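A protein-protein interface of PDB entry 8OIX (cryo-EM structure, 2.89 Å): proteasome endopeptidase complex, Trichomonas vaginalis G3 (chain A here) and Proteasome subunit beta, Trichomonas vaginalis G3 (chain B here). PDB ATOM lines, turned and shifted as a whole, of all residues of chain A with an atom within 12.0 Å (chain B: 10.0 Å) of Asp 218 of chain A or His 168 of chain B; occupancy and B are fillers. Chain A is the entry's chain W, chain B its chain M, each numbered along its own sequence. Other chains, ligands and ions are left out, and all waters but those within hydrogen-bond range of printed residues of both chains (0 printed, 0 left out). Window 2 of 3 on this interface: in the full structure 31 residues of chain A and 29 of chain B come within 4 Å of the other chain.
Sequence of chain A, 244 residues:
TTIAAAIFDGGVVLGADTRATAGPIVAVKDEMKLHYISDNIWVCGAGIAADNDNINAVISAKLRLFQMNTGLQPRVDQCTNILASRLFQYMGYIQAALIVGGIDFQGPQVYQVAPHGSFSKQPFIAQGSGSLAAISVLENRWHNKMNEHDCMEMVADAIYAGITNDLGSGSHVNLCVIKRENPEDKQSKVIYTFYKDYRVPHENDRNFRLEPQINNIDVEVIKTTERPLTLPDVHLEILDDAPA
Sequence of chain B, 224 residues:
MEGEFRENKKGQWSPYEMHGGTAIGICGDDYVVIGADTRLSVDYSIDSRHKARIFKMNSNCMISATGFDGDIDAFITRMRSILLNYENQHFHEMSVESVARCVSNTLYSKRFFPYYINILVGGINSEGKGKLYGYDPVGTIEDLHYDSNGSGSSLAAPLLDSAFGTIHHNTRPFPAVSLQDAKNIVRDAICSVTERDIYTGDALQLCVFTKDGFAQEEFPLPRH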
ATOM      1  N   GLN A 213      -0.450   3.011  -1.652  1.00  0.00           N
ATOM      2  CA  GLN A 213      -1.202   3.230  -2.881  1.00  0.00           C
ATOM      3  C   GLN A 213      -2.409   4.113  -2.594  1.00  0.00           C
ATOM      4  O   GLN A 213      -3.294   3.736  -1.819  1.00  0.00           O
ATOM      5  CB  GLN A 213      -1.637   1.898  -3.484  1.00  0.00           C
ATOM      6  CG  GLN A 213      -2.405   2.035  -4.786  1.00  0.00           C
ATOM      7  CD  GLN A 213      -3.050   0.735  -5.215  1.00  0.00           C
ATOM      8  OE1 GLN A 213      -2.399  -0.308  -5.261  1.00  0.00           O
ATOM      9  NE2 GLN A 213      -4.339   0.790  -5.531  1.00  0.00           N
ATOM     10  N   ILE A 214      -2.445   5.287  -3.217  1.00  0.00           N
ATOM     11  CA  ILE A 214      -3.531   6.235  -3.001  1.00  0.00           C
ATOM     12  C   ILE A 214      -4.704   5.851  -3.892  1.00  0.00           C
ATOM     13  O   ILE A 214      -4.568   5.767  -5.117  1.00  0.00           O
ATOM     14  CB  ILE A 214      -3.071   7.674  -3.275  1.00  0.00           C
ATOM     15  CG1 ILE A 214      -1.821   7.991  -2.453  1.00  0.00           C
ATOM     16  CG2 ILE A 214      -4.187   8.659  -2.966  1.00  0.00           C
ATOM     17  CD1 ILE A 214      -1.359   9.423  -2.564  1.00  0.00           C
ATOM     18  N   ASN A 215      -5.861   5.617  -3.276  1.00  0.00           N
ATOM     19  CA  ASN A 215      -7.065   5.249  -4.007  1.00  0.00           C
ATOM     20  C   ASN A 215      -8.266   5.833  -3.280  1.00  0.00           C
ATOM     21  O   ASN A 215      -8.431   5.608  -2.078  1.00  0.00           O
ATOM     22  CB  ASN A 215      -7.195   3.727  -4.131  1.00  0.00           C
ATOM     23  CG  ASN A 215      -8.388   3.307  -4.968  1.00  0.00           C
ATOM     24  OD1 ASN A 215      -9.537   3.453  -4.553  1.00  0.00           O
ATOM     25  ND2 ASN A 215      -8.119   2.779  -6.155  1.00  0.00           N
ATOM     26  N   ASN A 216      -9.096   6.579  -4.008  1.00  0.00           N
ATOM     27  CA  ASN A 216     -10.329   7.135  -3.461  1.00  0.00           C
ATOM     28  C   ASN A 216     -11.563   6.596  -4.178  1.00  0.00           C
ATOM     29  O   ASN A 216     -12.589   7.275  -4.254  1.00  0.00           O
ATOM     30  CB  ASN A 216     -10.305   8.661  -3.514  1.00  0.00           C
ATOM     31  CG  ASN A 216      -9.365   9.266  -2.491  1.00  0.00           C
ATOM     32  OD1 ASN A 216      -9.781   9.643  -1.395  1.00  0.00           O
ATOM     33  ND2 ASN A 216      -8.090   9.366  -2.844  1.00  0.00           N
ATOM     34  N   ILE A 217     -11.481   5.380  -4.711  1.00  0.00           N
ATOM     35  CA  ILE A 217     -12.633   4.693  -5.282  1.00  0.00           C
ATOM     36  C   ILE A 217     -13.149   3.695  -4.257  1.00  0.00           C
ATOM     37  O   ILE A 217     -12.387   2.860  -3.755  1.00  0.00           O
ATOM     38  CB  ILE A 217     -12.278   3.993  -6.605  1.00  0.00           C
ATOM     39  CG1 ILE A 217     -12.226   5.004  -7.750  1.00  0.00           C
ATOM     40  CG2 ILE A 217     -13.279   2.892  -6.918  1.00  0.00           C
ATOM     41  CD1 ILE A 217     -11.819   4.401  -9.073  1.00  0.00           C
ATOM     42  N   ASP A 218     -14.436   3.787  -3.936  1.00  0.00           N
ATOM     43  CA  ASP A 218     -15.075   2.902  -2.973  1.00  0.00           C
ATOM     44  C   ASP A 218     -16.010   1.951  -3.706  1.00  0.00           C
ATOM     45  O   ASP A 218     -16.829   2.386  -4.524  1.00  0.00           O
ATOM     46  CB  ASP A 218     -15.840   3.703  -1.918  1.00  0.00           C
ATOM     47  CG  ASP A 218     -14.917   4.468  -0.989  1.00  0.00           C
ATOM     48  OD1 ASP A 218     -13.800   3.974  -0.721  1.00  0.00           O
ATOM     49  OD2 ASP A 218     -15.303   5.560  -0.525  1.00  0.00           O
ATOM     50  N   VAL A 219     -15.882   0.661  -3.418  1.00  0.00           N
ATOM     51  CA  VAL A 219     -16.671  -0.370  -4.084  1.00  0.00           C
ATOM     52  C   VAL A 219     -17.977  -0.564  -3.330  1.00  0.00           C
ATOM     53  O   VAL A 219     -17.976  -0.874  -2.134  1.00  0.00           O
ATOM     54  CB  VAL A 219     -15.897  -1.692  -4.171  1.00  0.00           C
ATOM     55  CG1 VAL A 219     -16.722  -2.733  -4.905  1.00  0.00           C
ATOM     56  CG2 VAL A 219     -14.578  -1.476  -4.859  1.00  0.00           C
ATOM     57  N   GLU A 220     -19.091  -0.383  -4.029  1.00  0.00           N
ATOM     58  CA  GLU A 220     -20.411  -0.694  -3.499  1.00  0.00           C
ATOM     59  C   GLU A 220     -20.889  -1.976  -4.170  1.00  0.00           C
ATOM     60  O   GLU A 220     -20.999  -2.032  -5.399  1.00  0.00           O
ATOM     61  CB  GLU A 220     -21.381   0.460  -3.741  1.00  0.00           C
ATOM     62  CG  GLU A 220     -20.916   1.773  -3.122  1.00  0.00           C
ATOM     63  CD  GLU A 220     -21.913   2.901  -3.299  1.00  0.00           C
ATOM     64  OE1 GLU A 220     -23.121   2.618  -3.422  1.00  0.00           O
ATOM     65  OE2 GLU A 220     -21.486   4.075  -3.317  1.00  0.00           O
ATOM     66  N   VAL A 221     -21.153  -3.002  -3.370  1.00  0.00           N
ATOM     67  CA  VAL A 221     -21.482  -4.326  -3.885  1.00  0.00           C
ATOM     68  C   VAL A 221     -22.999  -4.458  -3.954  1.00  0.00           C
ATOM     69  O   VAL A 221     -23.682  -4.443  -2.927  1.00  0.00           O
ATOM     70  CB  VAL A 221     -20.868  -5.433  -3.023  1.00  0.00           C
ATOM     71  CG1 VAL A 221     -21.305  -6.786  -3.533  1.00  0.00           C
ATOM     72  CG2 VAL A 221     -19.352  -5.321  -3.024  1.00  0.00           C
ATOM     73  N   ILE A 222     -23.527  -4.585  -5.173  1.00  0.00           N
ATOM     74  CA  ILE A 222     -24.966  -4.762  -5.350  1.00  0.00           C
ATOM     75  C   ILE A 222     -25.418  -6.090  -4.760  1.00  0.00           C
ATOM     76  O   ILE A 222     -26.395  -6.154  -4.005  1.00  0.00           O
ATOM     77  CB  ILE A 222     -25.336  -4.663  -6.841  1.00  0.00           C
ATOM     78  CG1 ILE A 222     -24.828  -3.352  -7.439  1.00  0.00           C
ATOM     79  CG2 ILE A 222     -26.841  -4.790  -7.025  1.00  0.00           C
ATOM     80  CD1 ILE A 222     -25.328  -2.135  -6.716  1.00  0.00           C
ATOM     81  N   TYR B 146      -7.472  17.385 -12.213  1.00  0.00           N
ATOM     82  CA  TYR B 146      -6.426  16.571 -12.805  1.00  0.00           C
ATOM     83  C   TYR B 146      -6.790  16.301 -14.256  1.00  0.00           C
ATOM     84  O   TYR B 146      -7.955  16.386 -14.652  1.00  0.00           O
ATOM     85  CB  TYR B 146      -6.225  15.258 -12.042  1.00  0.00           C
ATOM     86  CG  TYR B 146      -7.433  14.350 -12.053  1.00  0.00           C
ATOM     87  CD1 TYR B 146      -7.681  13.498 -13.119  1.00  0.00           C
ATOM     88  CD2 TYR B 146      -8.323  14.343 -10.992  1.00  0.00           C
ATOM     89  CE1 TYR B 146      -8.778  12.671 -13.130  1.00  0.00           C
ATOM     90  CE2 TYR B 146      -9.422  13.519 -10.993  1.00  0.00           C
ATOM     91  CZ  TYR B 146      -9.646  12.685 -12.064  1.00  0.00           C
ATOM     92  OH  TYR B 146     -10.743  11.860 -12.068  1.00  0.00           O
ATOM     93  N   ALA B 157      -5.464   8.105 -17.103  1.00  0.00           N
ATOM     94  CA  ALA B 157      -6.688   8.682 -16.552  1.00  0.00           C
ATOM     95  C   ALA B 157      -7.319   7.820 -15.465  1.00  0.00           C
ATOM     96  O   ALA B 157      -7.701   8.375 -14.420  1.00  0.00           O
ATOM     97  CB  ALA B 157      -7.671   8.980 -17.688  1.00  0.00           C
ATOM     98  N   PRO B 158      -7.479   6.500 -15.627  1.00  0.00           N
ATOM     99  CA  PRO B 158      -7.962   5.689 -14.497  1.00  0.00           C
ATOM    100  C   PRO B 158      -7.080   5.766 -13.270  1.00  0.00           C
ATOM    101  O   PRO B 158      -7.592   5.661 -12.152  1.00  0.00           O
ATOM    102  CB  PRO B 158      -7.992   4.268 -15.072  1.00  0.00           C
ATOM    103  CG  PRO B 158      -8.144   4.457 -16.507  1.00  0.00           C
ATOM    104  CD  PRO B 158      -7.414   5.705 -16.862  1.00  0.00           C
ATOM    105  N   LEU B 160      -5.519   8.409 -12.116  1.00  0.00           N
ATOM    106  CA  LEU B 160      -5.919   9.614 -11.402  1.00  0.00           C
ATOM    107  C   LEU B 160      -7.334   9.483 -10.853  1.00  0.00           C
ATOM    108  O   LEU B 160      -7.623   9.956  -9.748  1.00  0.00           O
ATOM    109  CB  LEU B 160      -5.804  10.819 -12.327  1.00  0.00           C
ATOM    110  CG  LEU B 160      -4.443  10.983 -13.002  1.00  0.00           C
ATOM    111  CD1 LEU B 160      -4.521  11.994 -14.133  1.00  0.00           C
ATOM    112  CD2 LEU B 160      -3.400  11.391 -11.980  1.00  0.00           C
ATOM    113  N   ASP B 161      -8.228   8.842 -11.610  1.00  0.00           N
ATOM    114  CA  ASP B 161      -9.583   8.619 -11.116  1.00  0.00           C
ATOM    115  C   ASP B 161      -9.570   7.803  -9.833  1.00  0.00           C
ATOM    116  O   ASP B 161     -10.303   8.107  -8.889  1.00  0.00           O
ATOM    117  CB  ASP B 161     -10.425   7.917 -12.179  1.00  0.00           C
ATOM    118  CG  ASP B 161     -10.522   8.710 -13.457  1.00  0.00           C
ATOM    119  OD1 ASP B 161     -10.030   9.855 -13.486  1.00  0.00           O
ATOM    120  OD2 ASP B 161     -11.099   8.192 -14.432  1.00  0.00           O
ATOM    121  N   SER B 162      -8.745   6.759  -9.782  1.00  0.00           N
ATOM    122  CA  SER B 162      -8.626   5.977  -8.560  1.00  0.00           C
ATOM    123  C   SER B 162      -7.998   6.798  -7.445  1.00  0.00           C
ATOM    124  O   SER B 162      -8.479   6.775  -6.307  1.00  0.00           O
ATOM    125  CB  SER B 162      -7.814   4.713  -8.825  1.00  0.00           C
ATOM    126  OG  SER B 162      -8.393   3.963  -9.875  1.00  0.00           O
ATOM    127  N   ALA B 163      -6.933   7.543  -7.756  1.00  0.00           N
ATOM    128  CA  ALA B 163      -6.268   8.339  -6.733  1.00  0.00           C
ATOM    129  C   ALA B 163      -7.203   9.369  -6.111  1.00  0.00           C
ATOM    130  O   ALA B 163      -7.066   9.690  -4.926  1.00  0.00           O
ATOM    131  CB  ALA B 163      -5.039   9.030  -7.324  1.00  0.00           C
ATOM    132  N   PHE B 164      -8.156   9.895  -6.882  1.00  0.00           N
ATOM    133  CA  PHE B 164      -9.017  10.962  -6.393  1.00  0.00           C
ATOM    134  C   PHE B 164     -10.502  10.630  -6.362  1.00  0.00           C
ATOM    135  O   PHE B 164     -11.230  11.243  -5.573  1.00  0.00           O
ATOM    136  CB  PHE B 164      -8.811  12.234  -7.229  1.00  0.00           C
ATOM    137  CG  PHE B 164      -7.372  12.631  -7.368  1.00  0.00           C
ATOM    138  CD1 PHE B 164      -6.657  13.073  -6.271  1.00  0.00           C
ATOM    139  CD2 PHE B 164      -6.734  12.564  -8.592  1.00  0.00           C
ATOM    140  CE1 PHE B 164      -5.334  13.435  -6.395  1.00  0.00           C
ATOM    141  CE2 PHE B 164      -5.413  12.926  -8.719  1.00  0.00           C
ATOM    142  CZ  PHE B 164      -4.713  13.362  -7.617  1.00  0.00           C
ATOM    143  N   GLY B 165     -10.975   9.692  -7.178  1.00  0.00           N
ATOM    144  CA  GLY B 165     -12.392   9.383  -7.195  1.00  0.00           C
ATOM    145  C   GLY B 165     -13.272  10.435  -7.823  1.00  0.00           C
ATOM    146  O   GLY B 165     -14.496  10.358  -7.686  1.00  0.00           O
ATOM    147  N   THR B 166     -12.688  11.423  -8.506  1.00  0.00           N
ATOM    148  CA  THR B 166     -13.485  12.511  -9.061  1.00  0.00           C
ATOM    149  C   THR B 166     -14.390  12.025 -10.186  1.00  0.00           C
ATOM    150  O   THR B 166     -15.538  12.465 -10.299  1.00  0.00           O
ATOM    151  CB  THR B 166     -12.569  13.631  -9.552  1.00  0.00           C
ATOM    152  OG1 THR B 166     -11.729  14.064  -8.475  1.00  0.00           O
ATOM    153  CG2 THR B 166     -13.386  14.814 -10.054  1.00  0.00           C
ATOM    154  N   ILE B 167     -13.895  11.117 -11.028  1.00  0.00           N
ATOM    155  CA  ILE B 167     -14.736  10.569 -12.087  1.00  0.00           C
ATOM    156  C   ILE B 167     -15.807   9.661 -11.498  1.00  0.00           C
ATOM    157  O   ILE B 167     -16.960   9.667 -11.945  1.00  0.00           O
ATOM    158  CB  ILE B 167     -13.872   9.837 -13.130  1.00  0.00           C
ATOM    159  CG1 ILE B 167     -13.056  10.843 -13.942  1.00  0.00           C
ATOM    160  CG2 ILE B 167     -14.739   9.008 -14.060  1.00  0.00           C
ATOM    161  CD1 ILE B 167     -13.860  11.660 -14.911  1.00  0.00           C
ATOM    162  N   HIS B 168     -15.446   8.876 -10.480  1.00  0.00           N
ATOM    163  CA  HIS B 168     -16.405   7.974  -9.848  1.00  0.00           C
ATOM    164  C   HIS B 168     -17.556   8.750  -9.224  1.00  0.00           C
ATOM    165  O   HIS B 168     -18.727   8.383  -9.376  1.00  0.00           O
ATOM    166  CB  HIS B 168     -15.692   7.123  -8.796  1.00  0.00           C
ATOM    167  CG  HIS B 168     -16.526   6.009  -8.245  1.00  0.00           C
ATOM    168  ND1 HIS B 168     -17.360   5.245  -9.032  1.00  0.00           N
ATOM    169  CD2 HIS B 168     -16.647   5.525  -6.988  1.00  0.00           C
ATOM    170  CE1 HIS B 168     -17.961   4.339  -8.282  1.00  0.00           C
ATOM    171  NE2 HIS B 168     -17.547   4.488  -7.037  1.00  0.00           N
ATOM    172  N   HIS B 169     -17.240   9.830  -8.515  1.00  0.00           N
ATOM    173  CA  HIS B 169     -18.238  10.695  -7.890  1.00  0.00           C
ATOM    174  C   HIS B 169     -17.879  12.135  -8.246  1.00  0.00           C
ATOM    175  O   HIS B 169     -16.973  12.723  -7.647  1.00  0.00           O
ATOM    176  CB  HIS B 169     -18.287  10.477  -6.385  1.00  0.00           C
ATOM    177  CG  HIS B 169     -18.881   9.162  -5.988  1.00  0.00           C
ATOM    178  ND1 HIS B 169     -18.253   8.289  -5.128  1.00  0.00           N
ATOM    179  CD2 HIS B 169     -20.050   8.573  -6.333  1.00  0.00           C
ATOM    180  CE1 HIS B 169     -19.007   7.217  -4.962  1.00  0.00           C
ATOM    181  NE2 HIS B 169     -20.104   7.365  -5.683  1.00  0.00           N
ATOM    182  N   ASN B 170     -18.593  12.694  -9.224  1.00  0.00           N
ATOM    183  CA  ASN B 170     -18.221  13.992  -9.776  1.00  0.00           C
ATOM    184  C   ASN B 170     -18.430  15.116  -8.771  1.00  0.00           C
ATOM    185  O   ASN B 170     -17.597  16.023  -8.665  1.00  0.00           O
ATOM    186  CB  ASN B 170     -19.020  14.264 -11.049  1.00  0.00           C
ATOM    187  CG  ASN B 170     -19.165  13.034 -11.917  1.00  0.00           C
ATOM    188  OD1 ASN B 170     -20.275  12.610 -12.228  1.00  0.00           O
ATOM    189  ND2 ASN B 170     -18.040  12.455 -12.315  1.00  0.00           N
ATOM    190  N   THR B 171     -19.532  15.076  -8.027  1.00  0.00           N
ATOM    191  CA  THR B 171     -19.946  16.209  -7.213  1.00  0.00           C
ATOM    192  C   THR B 171     -19.283  16.256  -5.844  1.00  0.00           C
ATOM    193  O   THR B 171     -19.401  17.276  -5.157  1.00  0.00           O
ATOM    194  CB  THR B 171     -21.464  16.188  -7.036  1.00  0.00           C
ATOM    195  OG1 THR B 171     -21.843  15.010  -6.315  1.00  0.00           O
ATOM    196  CG2 THR B 171     -22.129  16.162  -8.392  1.00  0.00           C
ATOM    197  N   ARG B 172     -18.598  15.197  -5.428  1.00  0.00           N
ATOM    198  CA  ARG B 172     -17.926  15.229  -4.143  1.00  0.00           C
ATOM    199  C   ARG B 172     -16.721  16.167  -4.203  1.00  0.00           C
ATOM    200  O   ARG B 172     -16.132  16.366  -5.269  1.00  0.00           O
ATOM    201  CB  ARG B 172     -17.485  13.827  -3.730  1.00  0.00           C
ATOM    202  CG  ARG B 172     -18.632  12.845  -3.598  1.00  0.00           C
ATOM    203  CD  ARG B 172     -18.179  11.536  -2.980  1.00  0.00           C
ATOM    204  NE  ARG B 172     -19.279  10.589  -2.853  1.00  0.00           N
ATOM    205  CZ  ARG B 172     -19.168   9.376  -2.330  1.00  0.00           C
ATOM    206  NH1 ARG B 172     -18.014   8.928  -1.864  1.00  0.00           N
ATOM    207  NH2 ARG B 172     -20.241   8.592  -2.275  1.00  0.00           N
ATOM    208  N   PHE B 174     -13.053  17.557  -4.208  1.00  0.00           N
ATOM    209  CA  PHE B 174     -11.792  16.956  -4.617  1.00  0.00           C
ATOM    210  C   PHE B 174     -10.897  16.764  -3.398  1.00  0.00           C
ATOM    211  O   PHE B 174     -10.697  17.712  -2.629  1.00  0.00           O
ATOM    212  CB  PHE B 174     -11.108  17.840  -5.656  1.00  0.00           C
ATOM    213  CG  PHE B 174      -9.829  17.273  -6.193  1.00  0.00           C
ATOM    214  CD1 PHE B 174      -9.847  16.221  -7.089  1.00  0.00           C
ATOM    215  CD2 PHE B 174      -8.610  17.808  -5.820  1.00  0.00           C
ATOM    216  CE1 PHE B 174      -8.672  15.704  -7.592  1.00  0.00           C
ATOM    217  CE2 PHE B 174      -7.433  17.295  -6.319  1.00  0.00           C
ATOM    218  CZ  PHE B 174      -7.464  16.243  -7.206  1.00  0.00           C
ATOM    219  N   PRO B 175     -10.360  15.563  -3.176  1.00  0.00           N
ATOM    220  CA  PRO B 175      -9.605  15.306  -1.943  1.00  0.00           C
ATOM    221  C   PRO B 175      -8.405  16.230  -1.803  1.00  0.00           C
ATOM    222  O   PRO B 175      -7.733  16.564  -2.780  1.00  0.00           O
ATOM    223  CB  PRO B 175      -9.176  13.841  -2.090  1.00  0.00           C
ATOM    224  CG  PRO B 175      -9.271  13.552  -3.553  1.00  0.00           C
ATOM    225  CD  PRO B 175     -10.408  14.382  -4.053  1.00  0.00           C
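Printed residues of chain B that touch a printed residue of chain A: Asp 161, Ser 162, Ala 163, Phe 164, Gly 165 and His 168.
Along chain B the printed residues that touch a printed residue of chain A span positions 161 to 168.
Of the 10 printed residues of chain A, 5 touch a printed residue of chain B.
The backbone carbonyl oxygen (O) of Ala 163 of chain B sits close to the side-chain amide nitrogen (ND2) of Asn 216 of chain A, at 2.3 Å.
NE2 of His 168 of chain B is in hydrogen-bond range of O of Asp 218 of chain A, at 3.4 Å.
The backbone NH (N) of Asn 216 of chain A lies close to the backbone carbonyl oxygen (O) of Ser 162 of chain B, at 2.4 Å.
Asp 218 of chain A touches one residue of chain B.
Of the printed residues of chain A, His 168 of chain B touches Asp 218.
Of chain B, only Asp 161 and Ser 162 come within 4 Å of Ile 217 of chain A.
No residue of chain B comes within 4 Å of Val 219 of chain A.
Of chain A, only Ile 217 comes within 4 Å of Asp 161 of chain B.
Gly 165 of chain B touches just one residue of chain A: Asn 216 (3.6 Å).
No residue of chain A comes within 4 Å of Thr 166 of chain B.
Ile 167 of chain B touches none of the printed residues of chain A.
His 169 of chain B touches none of the printed residues of chain A.
Asn 170 of chain B touches none of the printed residues of chain A.
Printed residues of chain B within 4 Å of Asn 215 of chain A: Ser 162.
Printed residues of chain A within 4 Å of Phe 164 of chain B: Asn 216 (3.4 Å).
Of the printed residues of chain A, Ser 162 of chain B touches Asn 215 (3.1 Å), Asn 216 (2.4 Å) and Ile 217 (3.5 Å).
Printed residues of chain B within 4 Å of Asn 216 of chain A: Ser 162 (2.4 Å), Ala 163 (2.3 Å), Phe 164 (3.4 Å) and Gly 165 (3.6 Å).
Val 221 of chain A touches none of the printed residues of chain B.
Ile 222 of chain A touches none of the printed residues of chain B.
The nearest residue of chain B that does not touch Asp 218 of chain A is Arg 172 of chain B (4.5 Å).
The side-chain amide oxygen (OD1) of Asn 215 of chain A is in hydrogen-bond range of the backbone NH (N) of Ile 217 of chain A, at 2.7 Å.
The side-chain carboxylate (OD1) of Asp 161 of chain B lies within hydrogen-bond range of the side-chain hydroxyl (OH) of Tyr 146 of chain B (2.6 Å).
The backbone carbonyl oxygen of Pro 158 of chain B sits at hydrogen-bond distance from the side-chain hydroxyl of Ser 162 of chain B (3.0 Å).
Ala 163 of chain B touches Ile 214 of chain A (CA to O, 3.5 Å).
CA of Asn 215 of chain A touches O of Ser 162 of chain B (3.1 Å).
CB of Asn 216 of chain A touches O of Phe 164 of chain B, 3.4 Å away.
Asn 216 of chain A touches Gly 165 of chain B.
Ile 217 of chain A touches Asp 161 of chain B (CG1 to O, 3.8 Å).
Ile 217 of chain A touches Ser 162 of chain B (CD1 to OG, 3.5 Å).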
